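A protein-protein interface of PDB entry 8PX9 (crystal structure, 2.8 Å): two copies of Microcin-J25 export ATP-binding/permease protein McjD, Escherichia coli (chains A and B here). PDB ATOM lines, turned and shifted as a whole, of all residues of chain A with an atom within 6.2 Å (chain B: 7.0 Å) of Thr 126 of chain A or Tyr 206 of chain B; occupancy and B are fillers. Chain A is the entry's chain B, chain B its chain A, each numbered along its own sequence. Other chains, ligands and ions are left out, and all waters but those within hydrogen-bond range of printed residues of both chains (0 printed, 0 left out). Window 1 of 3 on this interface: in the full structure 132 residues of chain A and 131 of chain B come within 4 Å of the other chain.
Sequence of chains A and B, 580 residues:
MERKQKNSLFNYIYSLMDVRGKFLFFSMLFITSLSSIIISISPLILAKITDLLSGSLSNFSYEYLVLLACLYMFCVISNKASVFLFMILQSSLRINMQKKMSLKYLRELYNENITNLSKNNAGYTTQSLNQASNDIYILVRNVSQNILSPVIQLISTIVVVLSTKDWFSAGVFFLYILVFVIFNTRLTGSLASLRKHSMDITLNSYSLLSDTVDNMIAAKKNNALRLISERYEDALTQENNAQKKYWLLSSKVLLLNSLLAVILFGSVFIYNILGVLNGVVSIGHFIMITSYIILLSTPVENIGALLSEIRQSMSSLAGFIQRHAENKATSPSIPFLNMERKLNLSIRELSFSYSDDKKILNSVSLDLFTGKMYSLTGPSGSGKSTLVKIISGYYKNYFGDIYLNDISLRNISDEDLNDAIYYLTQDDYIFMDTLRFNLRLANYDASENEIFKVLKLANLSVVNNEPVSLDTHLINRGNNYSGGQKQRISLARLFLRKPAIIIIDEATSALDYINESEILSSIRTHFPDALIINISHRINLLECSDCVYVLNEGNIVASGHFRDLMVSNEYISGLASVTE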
ATOM      1  N   TYR A 105     -26.268  10.276 -17.481  1.00  0.00           N
ATOM      2  CA  TYR A 105     -25.892  10.529 -16.093  1.00  0.00           C
ATOM      3  C   TYR A 105     -25.628  12.011 -15.841  1.00  0.00           C
ATOM      4  O   TYR A 105     -26.096  12.526 -14.829  1.00  0.00           O
ATOM      5  CB  TYR A 105     -24.646   9.719 -15.723  1.00  0.00           C
ATOM      6  CG  TYR A 105     -24.221   9.775 -14.265  1.00  0.00           C
ATOM      7  CD1 TYR A 105     -25.102   9.445 -13.223  1.00  0.00           C
ATOM      8  CD2 TYR A 105     -22.913  10.120 -13.928  1.00  0.00           C
ATOM      9  CE1 TYR A 105     -24.688   9.468 -11.894  1.00  0.00           C
ATOM     10  CE2 TYR A 105     -22.483  10.119 -12.606  1.00  0.00           C
ATOM     11  CZ  TYR A 105     -23.367   9.780 -11.587  1.00  0.00           C
ATOM     12  OH  TYR A 105     -22.956   9.782 -10.284  1.00  0.00           O
ATOM     13  N   ASN A 121     -19.565  14.344  -3.057  1.00  0.00           N
ATOM     14  CA  ASN A 121     -18.424  14.938  -3.747  1.00  0.00           C
ATOM     15  C   ASN A 121     -18.346  14.420  -5.184  1.00  0.00           C
ATOM     16  O   ASN A 121     -19.033  13.462  -5.513  1.00  0.00           O
ATOM     17  CB  ASN A 121     -17.120  14.657  -2.988  1.00  0.00           C
ATOM     18  CG  ASN A 121     -15.959  15.537  -3.417  1.00  0.00           C
ATOM     19  OD1 ASN A 121     -16.117  16.603  -4.017  1.00  0.00           O
ATOM     20  ND2 ASN A 121     -14.759  15.064  -3.195  1.00  0.00           N
ATOM     21  N   ALA A 122     -17.525  15.042  -6.049  1.00  0.00           N
ATOM     22  CA  ALA A 122     -17.291  14.582  -7.418  1.00  0.00           C
ATOM     23  C   ALA A 122     -16.587  13.222  -7.522  1.00  0.00           C
ATOM     24  O   ALA A 122     -16.911  12.458  -8.433  1.00  0.00           O
ATOM     25  CB  ALA A 122     -16.517  15.617  -8.198  1.00  0.00           C
ATOM     26  N   GLY A 123     -15.619  12.925  -6.638  1.00  0.00           N
ATOM     27  CA  GLY A 123     -14.984  11.609  -6.618  1.00  0.00           C
ATOM     28  C   GLY A 123     -15.979  10.465  -6.410  1.00  0.00           C
ATOM     29  O   GLY A 123     -15.859   9.417  -7.045  1.00  0.00           O
ATOM     30  N   TYR A 124     -16.967  10.708  -5.532  1.00  0.00           N
ATOM     31  CA  TYR A 124     -18.115   9.837  -5.326  1.00  0.00           C
ATOM     32  C   TYR A 124     -18.960   9.736  -6.591  1.00  0.00           C
ATOM     33  O   TYR A 124     -19.367   8.640  -6.935  1.00  0.00           O
ATOM     34  CB  TYR A 124     -18.930  10.362  -4.147  1.00  0.00           C
ATOM     35  CG  TYR A 124     -20.198   9.603  -3.800  1.00  0.00           C
ATOM     36  CD1 TYR A 124     -21.405   9.806  -4.490  1.00  0.00           C
ATOM     37  CD2 TYR A 124     -20.214   8.755  -2.693  1.00  0.00           C
ATOM     38  CE1 TYR A 124     -22.565   9.131  -4.124  1.00  0.00           C
ATOM     39  CE2 TYR A 124     -21.370   8.077  -2.316  1.00  0.00           C
ATOM     40  CZ  TYR A 124     -22.546   8.258  -3.037  1.00  0.00           C
ATOM     41  OH  TYR A 124     -23.678   7.588  -2.662  1.00  0.00           O
ATOM     42  N   THR A 125     -19.231  10.873  -7.239  1.00  0.00           N
ATOM     43  CA  THR A 125     -20.005  10.956  -8.479  1.00  0.00           C
ATOM     44  C   THR A 125     -19.367  10.156  -9.630  1.00  0.00           C
ATOM     45  O   THR A 125     -20.078   9.401 -10.303  1.00  0.00           O
ATOM     46  CB  THR A 125     -20.257  12.435  -8.846  1.00  0.00           C
ATOM     47  OG1 THR A 125     -20.817  13.116  -7.724  1.00  0.00           O
ATOM     48  CG2 THR A 125     -21.203  12.634 -10.003  1.00  0.00           C
ATOM     49  N   THR A 126     -18.051  10.323  -9.861  1.00  0.00           N
ATOM     50  CA  THR A 126     -17.345   9.610 -10.921  1.00  0.00           C
ATOM     51  C   THR A 126     -17.288   8.102 -10.643  1.00  0.00           C
ATOM     52  O   THR A 126     -17.465   7.316 -11.572  1.00  0.00           O
ATOM     53  CB  THR A 126     -15.932  10.159 -11.172  1.00  0.00           C
ATOM     54  OG1 THR A 126     -15.161  10.102  -9.973  1.00  0.00           O
ATOM     55  CG2 THR A 126     -15.936  11.563 -11.732  1.00  0.00           C
ATOM     56  N   GLN A 127     -17.044   7.711  -9.381  1.00  0.00           N
ATOM     57  CA  GLN A 127     -17.009   6.313  -8.981  1.00  0.00           C
ATOM     58  C   GLN A 127     -18.404   5.673  -8.974  1.00  0.00           C
ATOM     59  O   GLN A 127     -18.504   4.466  -9.162  1.00  0.00           O
ATOM     60  CB  GLN A 127     -16.303   6.164  -7.626  1.00  0.00           C
ATOM     61  CG  GLN A 127     -15.905   4.734  -7.275  1.00  0.00           C
ATOM     62  CD  GLN A 127     -14.948   4.116  -8.271  1.00  0.00           C
ATOM     63  OE1 GLN A 127     -14.028   4.775  -8.763  1.00  0.00           O
ATOM     64  NE2 GLN A 127     -15.174   2.849  -8.585  1.00  0.00           N
ATOM     65  N   SER A 128     -19.471   6.455  -8.750  1.00  0.00           N
ATOM     66  CA  SER A 128     -20.846   5.973  -8.824  1.00  0.00           C
ATOM     67  C   SER A 128     -21.186   5.520 -10.242  1.00  0.00           C
ATOM     68  O   SER A 128     -21.865   4.508 -10.388  1.00  0.00           O
ATOM     69  CB  SER A 128     -21.836   7.020  -8.342  1.00  0.00           C
ATOM     70  OG  SER A 128     -21.704   7.261  -6.954  1.00  0.00           O
ATOM     71  N   LEU A 129     -20.726   6.282 -11.254  1.00  0.00           N
ATOM     72  CA  LEU A 129     -20.853   5.920 -12.661  1.00  0.00           C
ATOM     73  C   LEU A 129     -20.073   4.645 -12.952  1.00  0.00           C
ATOM     74  O   LEU A 129     -20.585   3.821 -13.705  1.00  0.00           O
ATOM     75  CB  LEU A 129     -20.338   7.055 -13.558  1.00  0.00           C
ATOM     76  CG  LEU A 129     -20.413   6.846 -15.078  1.00  0.00           C
ATOM     77  CD1 LEU A 129     -21.853   6.937 -15.563  1.00  0.00           C
ATOM     78  CD2 LEU A 129     -19.496   7.823 -15.803  1.00  0.00           C
ATOM     79  N   ASN A 130     -18.853   4.501 -12.391  1.00  0.00           N
ATOM     80  CA  ASN A 130     -18.023   3.304 -12.535  1.00  0.00           C
ATOM     81  C   ASN A 130     -18.745   2.053 -12.038  1.00  0.00           C
ATOM     82  O   ASN A 130     -18.750   1.049 -12.735  1.00  0.00           O
ATOM     83  CB  ASN A 130     -16.669   3.427 -11.803  1.00  0.00           C
ATOM     84  CG  ASN A 130     -15.587   4.125 -12.601  1.00  0.00           C
ATOM     85  OD1 ASN A 130     -15.546   4.026 -13.816  1.00  0.00           O
ATOM     86  ND2 ASN A 130     -14.657   4.795 -11.941  1.00  0.00           N
ATOM     87  N   GLN A 131     -19.315   2.121 -10.830  1.00  0.00           N
ATOM     88  CA  GLN A 131     -20.043   1.016 -10.225  1.00  0.00           C
ATOM     89  C   GLN A 131     -21.307   0.674 -11.022  1.00  0.00           C
ATOM     90  O   GLN A 131     -21.576  -0.501 -11.218  1.00  0.00           O
ATOM     91  CB  GLN A 131     -20.370   1.324  -8.758  1.00  0.00           C
ATOM     92  CG  GLN A 131     -19.152   1.317  -7.832  1.00  0.00           C
ATOM     93  CD  GLN A 131     -19.485   1.371  -6.351  1.00  0.00           C
ATOM     94  OE1 GLN A 131     -20.611   1.669  -5.930  1.00  0.00           O
ATOM     95  NE2 GLN A 131     -18.483   1.068  -5.531  1.00  0.00           N
ATOM     96  N   SER A 133     -22.055   1.498 -14.304  1.00  0.00           N
ATOM     97  CA  SER A 133     -21.712   1.043 -15.651  1.00  0.00           C
ATOM     98  C   SER A 133     -21.236  -0.417 -15.652  1.00  0.00           C
ATOM     99  O   SER A 133     -21.525  -1.150 -16.592  1.00  0.00           O
ATOM    100  CB  SER A 133     -20.678   1.942 -16.271  1.00  0.00           C
ATOM    101  OG  SER A 133     -19.499   1.963 -15.474  1.00  0.00           O
ATOM    102  N   ASN B 121      -6.731  16.940 -11.802  1.00  0.00           N
ATOM    103  CA  ASN B 121      -8.083  17.073 -11.193  1.00  0.00           C
ATOM    104  C   ASN B 121      -8.302  15.924 -10.202  1.00  0.00           C
ATOM    105  O   ASN B 121      -7.618  14.895 -10.340  1.00  0.00           O
ATOM    106  CB  ASN B 121      -9.182  17.105 -12.259  1.00  0.00           C
ATOM    107  CG  ASN B 121     -10.437  17.813 -11.798  1.00  0.00           C
ATOM    108  OD1 ASN B 121     -10.460  18.415 -10.726  1.00  0.00           O
ATOM    109  ND2 ASN B 121     -11.488  17.747 -12.600  1.00  0.00           N
ATOM    110  N   ALA B 122      -9.213  16.101  -9.241  1.00  0.00           N
ATOM    111  CA  ALA B 122      -9.524  15.023  -8.271  1.00  0.00           C
ATOM    112  C   ALA B 122     -10.106  13.823  -9.024  1.00  0.00           C
ATOM    113  O   ALA B 122      -9.653  12.692  -8.770  1.00  0.00           O
ATOM    114  CB  ALA B 122     -10.475  15.533  -7.219  1.00  0.00           C
ATOM    115  N   GLY B 123     -11.077  14.064  -9.911  1.00  0.00           N
ATOM    116  CA  GLY B 123     -11.652  12.989 -10.701  1.00  0.00           C
ATOM    117  C   GLY B 123     -10.576  12.235 -11.490  1.00  0.00           C
ATOM    118  O   GLY B 123     -10.616  11.012 -11.589  1.00  0.00           O
ATOM    119  N   TYR B 124      -9.593  12.999 -11.998  1.00  0.00           N
ATOM    120  CA  TYR B 124      -8.426  12.508 -12.697  1.00  0.00           C
ATOM    121  C   TYR B 124      -7.559  11.702 -11.735  1.00  0.00           C
ATOM    122  O   TYR B 124      -7.092  10.630 -12.085  1.00  0.00           O
ATOM    123  CB  TYR B 124      -7.654  13.688 -13.286  1.00  0.00           C
ATOM    124  CG  TYR B 124      -6.349  13.357 -13.978  1.00  0.00           C
ATOM    125  CD1 TYR B 124      -5.161  13.197 -13.265  1.00  0.00           C
ATOM    126  CD2 TYR B 124      -6.299  13.270 -15.365  1.00  0.00           C
ATOM    127  CE1 TYR B 124      -3.972  12.900 -13.912  1.00  0.00           C
ATOM    128  CE2 TYR B 124      -5.111  12.978 -16.028  1.00  0.00           C
ATOM    129  CZ  TYR B 124      -3.941  12.791 -15.300  1.00  0.00           C
ATOM    130  OH  TYR B 124      -2.779  12.507 -15.967  1.00  0.00           O
ATOM    131  N   THR B 126      -8.450  10.211  -8.747  1.00  0.00           N
ATOM    132  CA  THR B 126      -9.098   8.975  -8.312  1.00  0.00           C
ATOM    133  C   THR B 126      -9.091   7.911  -9.423  1.00  0.00           C
ATOM    134  O   THR B 126      -8.883   6.732  -9.137  1.00  0.00           O
ATOM    135  CB  THR B 126     -10.521   9.219  -7.793  1.00  0.00           C
ATOM    136  OG1 THR B 126     -11.319   9.827  -8.814  1.00  0.00           O
ATOM    137  CG2 THR B 126     -10.545  10.044  -6.522  1.00  0.00           C
ATOM    138  N   GLN B 127      -9.309   8.331 -10.678  1.00  0.00           N
ATOM    139  CA  GLN B 127      -9.297   7.429 -11.823  1.00  0.00           C
ATOM    140  C   GLN B 127      -7.876   6.981 -12.190  1.00  0.00           C
ATOM    141  O   GLN B 127      -7.710   5.890 -12.731  1.00  0.00           O
ATOM    142  CB  GLN B 127     -10.017   8.061 -13.027  1.00  0.00           C
ATOM    143  CG  GLN B 127     -10.339   7.084 -14.159  1.00  0.00           C
ATOM    144  CD  GLN B 127     -11.236   5.941 -13.733  1.00  0.00           C
ATOM    145  OE1 GLN B 127     -12.190   6.111 -12.965  1.00  0.00           O
ATOM    146  NE2 GLN B 127     -10.940   4.749 -14.236  1.00  0.00           N
ATOM    147  N   ASN B 130      -7.333   4.027 -10.119  1.00  0.00           N
ATOM    148  CA  ASN B 130      -8.105   2.930 -10.709  1.00  0.00           C
ATOM    149  C   ASN B 130      -7.350   2.255 -11.852  1.00  0.00           C
ATOM    150  O   ASN B 130      -7.305   1.033 -11.919  1.00  0.00           O
ATOM    151  CB  ASN B 130      -9.458   3.426 -11.248  1.00  0.00           C
ATOM    152  CG  ASN B 130     -10.574   3.398 -10.235  1.00  0.00           C
ATOM    153  OD1 ASN B 130     -10.595   2.567  -9.339  1.00  0.00           O
ATOM    154  ND2 ASN B 130     -11.535   4.293 -10.382  1.00  0.00           N
ATOM    155  N   GLN B 131      -6.762   3.054 -12.748  1.00  0.00           N
ATOM    156  CA  GLN B 131      -6.015   2.547 -13.885  1.00  0.00           C
ATOM    157  C   GLN B 131      -4.731   1.852 -13.435  1.00  0.00           C
ATOM    158  O   GLN B 131      -4.415   0.785 -13.961  1.00  0.00           O
ATOM    159  CB  GLN B 131      -5.717   3.677 -14.880  1.00  0.00           C
ATOM    160  CG  GLN B 131      -6.951   4.160 -15.635  1.00  0.00           C
ATOM    161  CD  GLN B 131      -6.653   5.093 -16.787  1.00  0.00           C
ATOM    162  OE1 GLN B 131      -5.551   5.638 -16.923  1.00  0.00           O
ATOM    163  NE2 GLN B 131      -7.659   5.293 -17.639  1.00  0.00           N
ATOM    164  N   MET B 199      -6.454   5.093 -22.629  1.00  0.00           N
ATOM    165  CA  MET B 199      -6.557   5.254 -21.183  1.00  0.00           C
ATOM    166  C   MET B 199      -6.335   6.700 -20.746  1.00  0.00           C
ATOM    167  O   MET B 199      -6.899   7.117 -19.741  1.00  0.00           O
ATOM    168  CB  MET B 199      -5.542   4.366 -20.475  1.00  0.00           C
ATOM    169  CG  MET B 199      -5.971   2.948 -20.360  1.00  0.00           C
ATOM    170  SD  MET B 199      -4.538   1.960 -19.854  1.00  0.00           S
ATOM    171  CE  MET B 199      -4.681   2.058 -18.074  1.00  0.00           C
ATOM    172  N   ILE B 201      -7.073   9.415 -22.687  1.00  0.00           N
ATOM    173  CA  ILE B 201      -8.301  10.106 -23.089  1.00  0.00           C
ATOM    174  C   ILE B 201      -9.435   9.807 -22.089  1.00  0.00           C
ATOM    175  O   ILE B 201     -10.234  10.693 -21.785  1.00  0.00           O
ATOM    176  CB  ILE B 201      -8.680   9.798 -24.563  1.00  0.00           C
ATOM    177  CG1 ILE B 201      -7.591  10.304 -25.516  1.00  0.00           C
ATOM    178  CG2 ILE B 201     -10.034  10.408 -24.941  1.00  0.00           C
ATOM    179  CD1 ILE B 201      -7.695   9.786 -26.941  1.00  0.00           C
ATOM    180  N   THR B 202      -9.448   8.586 -21.528  1.00  0.00           N
ATOM    181  CA  THR B 202     -10.389   8.167 -20.501  1.00  0.00           C
ATOM    182  C   THR B 202     -10.205   9.012 -19.243  1.00  0.00           C
ATOM    183  O   THR B 202     -11.193   9.495 -18.714  1.00  0.00           O
ATOM    184  CB  THR B 202     -10.253   6.668 -20.228  1.00  0.00           C
ATOM    185  OG1 THR B 202     -10.591   5.970 -21.427  1.00  0.00           O
ATOM    186  CG2 THR B 202     -11.123   6.208 -19.082  1.00  0.00           C
ATOM    187  N   LEU B 203      -8.945   9.265 -18.827  1.00  0.00           N
ATOM    188  CA  LEU B 203      -8.638  10.127 -17.681  1.00  0.00           C
ATOM    189  C   LEU B 203      -9.135  11.552 -17.953  1.00  0.00           C
ATOM    190  O   LEU B 203      -9.718  12.181 -17.068  1.00  0.00           O
ATOM    191  CB  LEU B 203      -7.132  10.173 -17.399  1.00  0.00           C
ATOM    192  CG  LEU B 203      -6.524   8.967 -16.699  1.00  0.00           C
ATOM    193  CD1 LEU B 203      -5.007   9.103 -16.641  1.00  0.00           C
ATOM    194  CD2 LEU B 203      -7.092   8.799 -15.310  1.00  0.00           C
ATOM    195  N   ASN B 204      -8.923  12.041 -19.186  1.00  0.00           N
ATOM    196  CA  ASN B 204      -9.357  13.362 -19.611  1.00  0.00           C
ATOM    197  C   ASN B 204     -10.887  13.487 -19.570  1.00  0.00           C
ATOM    198  O   ASN B 204     -11.393  14.545 -19.221  1.00  0.00           O
ATOM    199  CB  ASN B 204      -8.779  13.684 -20.991  1.00  0.00           C
ATOM    200  CG  ASN B 204      -9.155  15.050 -21.533  1.00  0.00           C
ATOM    201  OD1 ASN B 204      -9.006  16.074 -20.862  1.00  0.00           O
ATOM    202  ND2 ASN B 204      -9.630  15.077 -22.769  1.00  0.00           N
ATOM    203  N   SER B 205     -11.616  12.406 -19.876  1.00  0.00           N
ATOM    204  CA  SER B 205     -13.078  12.386 -19.808  1.00  0.00           C
ATOM    205  C   SER B 205     -13.574  12.437 -18.365  1.00  0.00           C
ATOM    206  O   SER B 205     -14.611  13.048 -18.101  1.00  0.00           O
ATOM    207  CB  SER B 205     -13.639  11.160 -20.505  1.00  0.00           C
ATOM    208  OG  SER B 205     -13.382  11.219 -21.901  1.00  0.00           O
ATOM    209  N   TYR B 206     -12.839  11.798 -17.437  1.00  0.00           N
ATOM    210  CA  TYR B 206     -13.176  11.793 -16.014  1.00  0.00           C
ATOM    211  C   TYR B 206     -12.946  13.163 -15.382  1.00  0.00           C
ATOM    212  O   TYR B 206     -13.745  13.576 -14.541  1.00  0.00           O
ATOM    213  CB  TYR B 206     -12.407  10.696 -15.255  1.00  0.00           C
ATOM    214  CG  TYR B 206     -13.099   9.353 -15.330  1.00  0.00           C
ATOM    215  CD1 TYR B 206     -14.074   9.008 -14.400  1.00  0.00           C
ATOM    216  CD2 TYR B 206     -12.847   8.464 -16.367  1.00  0.00           C
ATOM    217  CE1 TYR B 206     -14.757   7.799 -14.482  1.00  0.00           C
ATOM    218  CE2 TYR B 206     -13.511   7.253 -16.464  1.00  0.00           C
ATOM    219  CZ  TYR B 206     -14.473   6.920 -15.516  1.00  0.00           C
ATOM    220  OH  TYR B 206     -15.161   5.743 -15.587  1.00  0.00           O
ATOM    221  N   SER B 207     -11.873  13.867 -15.797  1.00  0.00           N
ATOM    222  CA  SER B 207     -11.578  15.213 -15.311  1.00  0.00           C
ATOM    223  C   SER B 207     -12.662  16.197 -15.763  1.00  0.00           C
ATOM    224  O   SER B 207     -13.024  17.092 -15.005  1.00  0.00           O
ATOM    225  CB  SER B 207     -10.203  15.683 -15.771  1.00  0.00           C
ATOM    226  OG  SER B 207     -10.200  16.112 -17.129  1.00  0.00           O
ATOM    227  N   LEU B 208     -13.167  16.020 -16.999  1.00  0.00           N
ATOM    228  CA  LEU B 208     -14.218  16.853 -17.569  1.00  0.00           C
ATOM    229  C   LEU B 208     -15.559  16.602 -16.893  1.00  0.00           C
ATOM    230  O   LEU B 208     -16.323  17.544 -16.740  1.00  0.00           O
ATOM    231  CB  LEU B 208     -14.326  16.644 -19.081  1.00  0.00           C
ATOM    232  CG  LEU B 208     -13.115  17.141 -19.866  1.00  0.00           C
ATOM    233  CD1 LEU B 208     -13.211  16.698 -21.308  1.00  0.00           C
ATOM    234  CD2 LEU B 208     -12.948  18.637 -19.753  1.00  0.00           C
ATOM    235  N   LEU B 209     -15.844  15.360 -16.477  1.00  0.00           N
ATOM    236  CA  LEU B 209     -17.069  15.039 -15.749  1.00  0.00           C
ATOM    237  C   LEU B 209     -16.973  15.617 -14.332  1.00  0.00           C
ATOM    238  O   LEU B 209     -17.915  16.247 -13.852  1.00  0.00           O
ATOM    239  CB  LEU B 209     -17.287  13.521 -15.696  1.00  0.00           C
ATOM    240  CG  LEU B 209     -18.457  13.045 -14.822  1.00  0.00           C
ATOM    241  CD1 LEU B 209     -19.807  13.507 -15.380  1.00  0.00           C
ATOM    242  CD2 LEU B 209     -18.456  11.531 -14.635  1.00  0.00           C
ATOM    243  N   SER B 210     -15.819  15.426 -13.683  1.00  0.00           N
ATOM    244  CA  SER B 210     -15.559  15.917 -12.336  1.00  0.00           C
ATOM    245  C   SER B 210     -15.683  17.445 -12.285  1.00  0.00           C
ATOM    246  O   SER B 210     -16.276  17.993 -11.357  1.00  0.00           O
ATOM    247  CB  SER B 210     -14.182  15.459 -11.885  1.00  0.00           C
ATOM    248  OG  SER B 210     -13.997  15.612 -10.485  1.00  0.00           O
ATOM    249  N   ASP B 211     -15.150  18.120 -13.321  1.00  0.00           N
ATOM    250  CA  ASP B 211     -15.198  19.573 -13.470  1.00  0.00           C
ATOM    251  C   ASP B 211     -16.632  20.091 -13.643  1.00  0.00           C
ATOM    252  O   ASP B 211     -16.969  21.100 -13.043  1.00  0.00           O
ATOM    253  CB  ASP B 211     -14.315  20.003 -14.652  1.00  0.00           C
ATOM    254  CG  ASP B 211     -14.240  21.489 -14.883  1.00  0.00           C
ATOM    255  OD1 ASP B 211     -13.737  22.184 -13.996  1.00  0.00           O
ATOM    256  OD2 ASP B 211     -14.639  21.930 -15.965  1.00  0.00           O
ATOM    257  N   THR B 212     -17.471  19.401 -14.440  1.00  0.00           N
ATOM    258  CA  THR B 212     -18.866  19.802 -14.640  1.00  0.00           C
ATOM    259  C   THR B 212     -19.688  19.624 -13.360  1.00  0.00           C
ATOM    260  O   THR B 212     -20.485  20.495 -13.045  1.00  0.00           O
ATOM    261  CB  THR B 212     -19.517  19.080 -15.822  1.00  0.00           C
ATOM    262  OG1 THR B 212     -19.409  17.686 -15.587  1.00  0.00           O
ATOM    263  CG2 THR B 212     -18.892  19.386 -17.157  1.00  0.00           C
ATOM    264  N   VAL B 213     -19.486  18.522 -12.603  1.00  0.00           N
ATOM    265  CA  VAL B 213     -20.199  18.265 -11.342  1.00  0.00           C
ATOM    266  C   VAL B 213     -19.806  19.275 -10.234  1.00  0.00           C
ATOM    267  O   VAL B 213     -20.672  19.741  -9.487  1.00  0.00           O
ATOM    268  CB  VAL B 213     -20.052  16.793 -10.893  1.00  0.00           C
ATOM    269  CG1 VAL B 213     -20.659  16.550  -9.511  1.00  0.00           C
ATOM    270  CG2 VAL B 213     -20.662  15.845 -11.920  1.00  0.00           C
ATOM    271  N   TYR B 232     -18.806  17.339 -22.917  1.00  0.00           N
ATOM    272  CA  TYR B 232     -18.687  15.963 -22.448  1.00  0.00           C
ATOM    273  C   TYR B 232     -18.888  14.967 -23.586  1.00  0.00           C
ATOM    274  O   TYR B 232     -18.208  13.955 -23.630  1.00  0.00           O
ATOM    275  CB  TYR B 232     -19.672  15.700 -21.302  1.00  0.00           C
ATOM    276  CG  TYR B 232     -19.391  14.437 -20.516  1.00  0.00           C
ATOM    277  CD1 TYR B 232     -18.093  14.082 -20.138  1.00  0.00           C
ATOM    278  CD2 TYR B 232     -20.436  13.631 -20.091  1.00  0.00           C
ATOM    279  CE1 TYR B 232     -17.853  12.948 -19.381  1.00  0.00           C
ATOM    280  CE2 TYR B 232     -20.201  12.486 -19.338  1.00  0.00           C
ATOM    281  CZ  TYR B 232     -18.907  12.135 -18.992  1.00  0.00           C
ATOM    282  OH  TYR B 232     -18.666  10.987 -18.286  1.00  0.00           O
ATOM    283  N   ALA B 235     -15.769  14.735 -25.579  1.00  0.00           N
ATOM    284  CA  ALA B 235     -14.782  13.983 -24.812  1.00  0.00           C
ATOM    285  C   ALA B 235     -15.050  12.483 -24.928  1.00  0.00           C
ATOM    286  O   ALA B 235     -14.108  11.703 -25.002  1.00  0.00           O
ATOM    287  CB  ALA B 235     -14.831  14.397 -23.357  1.00  0.00           C
ATOM    288  N   GLU B 239     -12.997   9.415 -26.803  1.00  0.00           N
ATOM    289  CA  GLU B 239     -12.813   8.200 -26.018  1.00  0.00           C
ATOM    290  C   GLU B 239     -13.236   6.980 -26.840  1.00  0.00           C
ATOM    291  O   GLU B 239     -12.524   5.981 -26.852  1.00  0.00           O
ATOM    292  CB  GLU B 239     -13.628   8.288 -24.712  1.00  0.00           C
ATOM    293  CG  GLU B 239     -13.159   7.367 -23.599  1.00  0.00           C
ATOM    294  CD  GLU B 239     -14.090   7.318 -22.394  1.00  0.00           C
ATOM    295  OE1 GLU B 239     -15.319   7.277 -22.601  1.00  0.00           O
ATOM    296  OE2 GLU B 239     -13.581   7.260 -21.250  1.00  0.00           O
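Printed residues of chain A that touch a printed residue of chain B: Ala 122, Thr 125, Thr 126, Gln 127 and Asn 130. Hydrophobic or aromatic side chains of chain A that line the printed part of chain B: Ala 122. Among the printed residues, 8 pairs touch across the chains. Among the printed residues, no Asp or Glu carboxylate lies within 4 Å of a Lys or Arg side-chain nitrogen of the other chain.
Thr 126 of chain A touches just these residues of chain B: Tyr 206 and Leu 209. Of chain A, only Thr 126 (3.9 Å) and Asn 130 (2.5 Å) come within 4 Å of Tyr 206 of chain B. Of the printed residues of chain A, Gln 127 of chain B touches Asn 130. Of the printed residues of chain A, Asn 130 of chain B touches Gln 127 (3.0 Å) and Asn 130 (3.5 Å). Of the printed residues of chain B, Gln 127 of chain A touches Asn 130. Gly 123 of chain B touches none of the printed residues of chain A. Ser 205 of chain B touches none of the printed residues of chain A. The nearest residue of chain A that does not touch Tyr 206 of chain B is Leu 129 of chain A (4.8 Å). The nearest printed residue of chain A that does not touch Val 213 of chain B is Ala 122 of chain A (4.4 Å).
CB of Ala 122 of chain A touches OG of Ser 210 of chain B, 3.4 Å away. Val 213 of chain B touches Thr 125 of chain A. Thr 126 of chain A touches Tyr 206 of chain B. Leu 209 of chain B touches Thr 126 of chain A (CD2 to CG2, 3.8 Å). ND2 of Asn 130 of chain A touches ND2 of Asn 130 of chain B (3.5 Å).
The backbone carbonyl oxygen (O) of Asn 130 of chain A lies within hydrogen-bond range of the side-chain hydroxyl (OG) of Ser 133 of chain A (3.0 Å). ND2 of Asn 130 of chain A is in hydrogen-bond range of OE1 of Gln 127 of chain A (3.2 Å). The side-chain amide oxygen (OE1) of Gln 127 of chain B sits at hydrogen-bond distance from the side-chain amide nitrogen (ND2) of Asn 130 of chain B (3.2 Å). O of Gly 123 of chain A sits at hydrogen-bond distance from OG1 of Thr 126 of chain A (3.1 Å). O of Ala 122 of chain A sits at hydrogen-bond distance from OG1 of Thr 126 of chain A, at 3.3 Å. The side-chain hydroxyl (OH) of Tyr 105 of chain A is in hydrogen-bond range of the backbone carbonyl oxygen (O) of Thr 125 of chain A (2.9 Å).
The side-chain hydroxyl (OH) of Tyr 206 of chain B lies within hydrogen-bond range of the side-chain amide oxygen (OD1) of Asn 130 of chain A (2.5 Å). The side-chain amide nitrogen of Asn 130 of chain B is in hydrogen-bond range of the side-chain amide oxygen of Gln 127 of chain A. The side-chain amide oxygen of Gln 127 of chain B is in hydrogen-bond range of the side-chain amide nitrogen of Asn 130 of chain A (3.0 Å).
Gln 127 of chain A touches Asn 130 of chain B, and with the chains exchanged Asn 130 of chain A touches Gln 127 of chain B. Asn 130 of chain B touches its own counterpart, Asn 130 of chain A.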
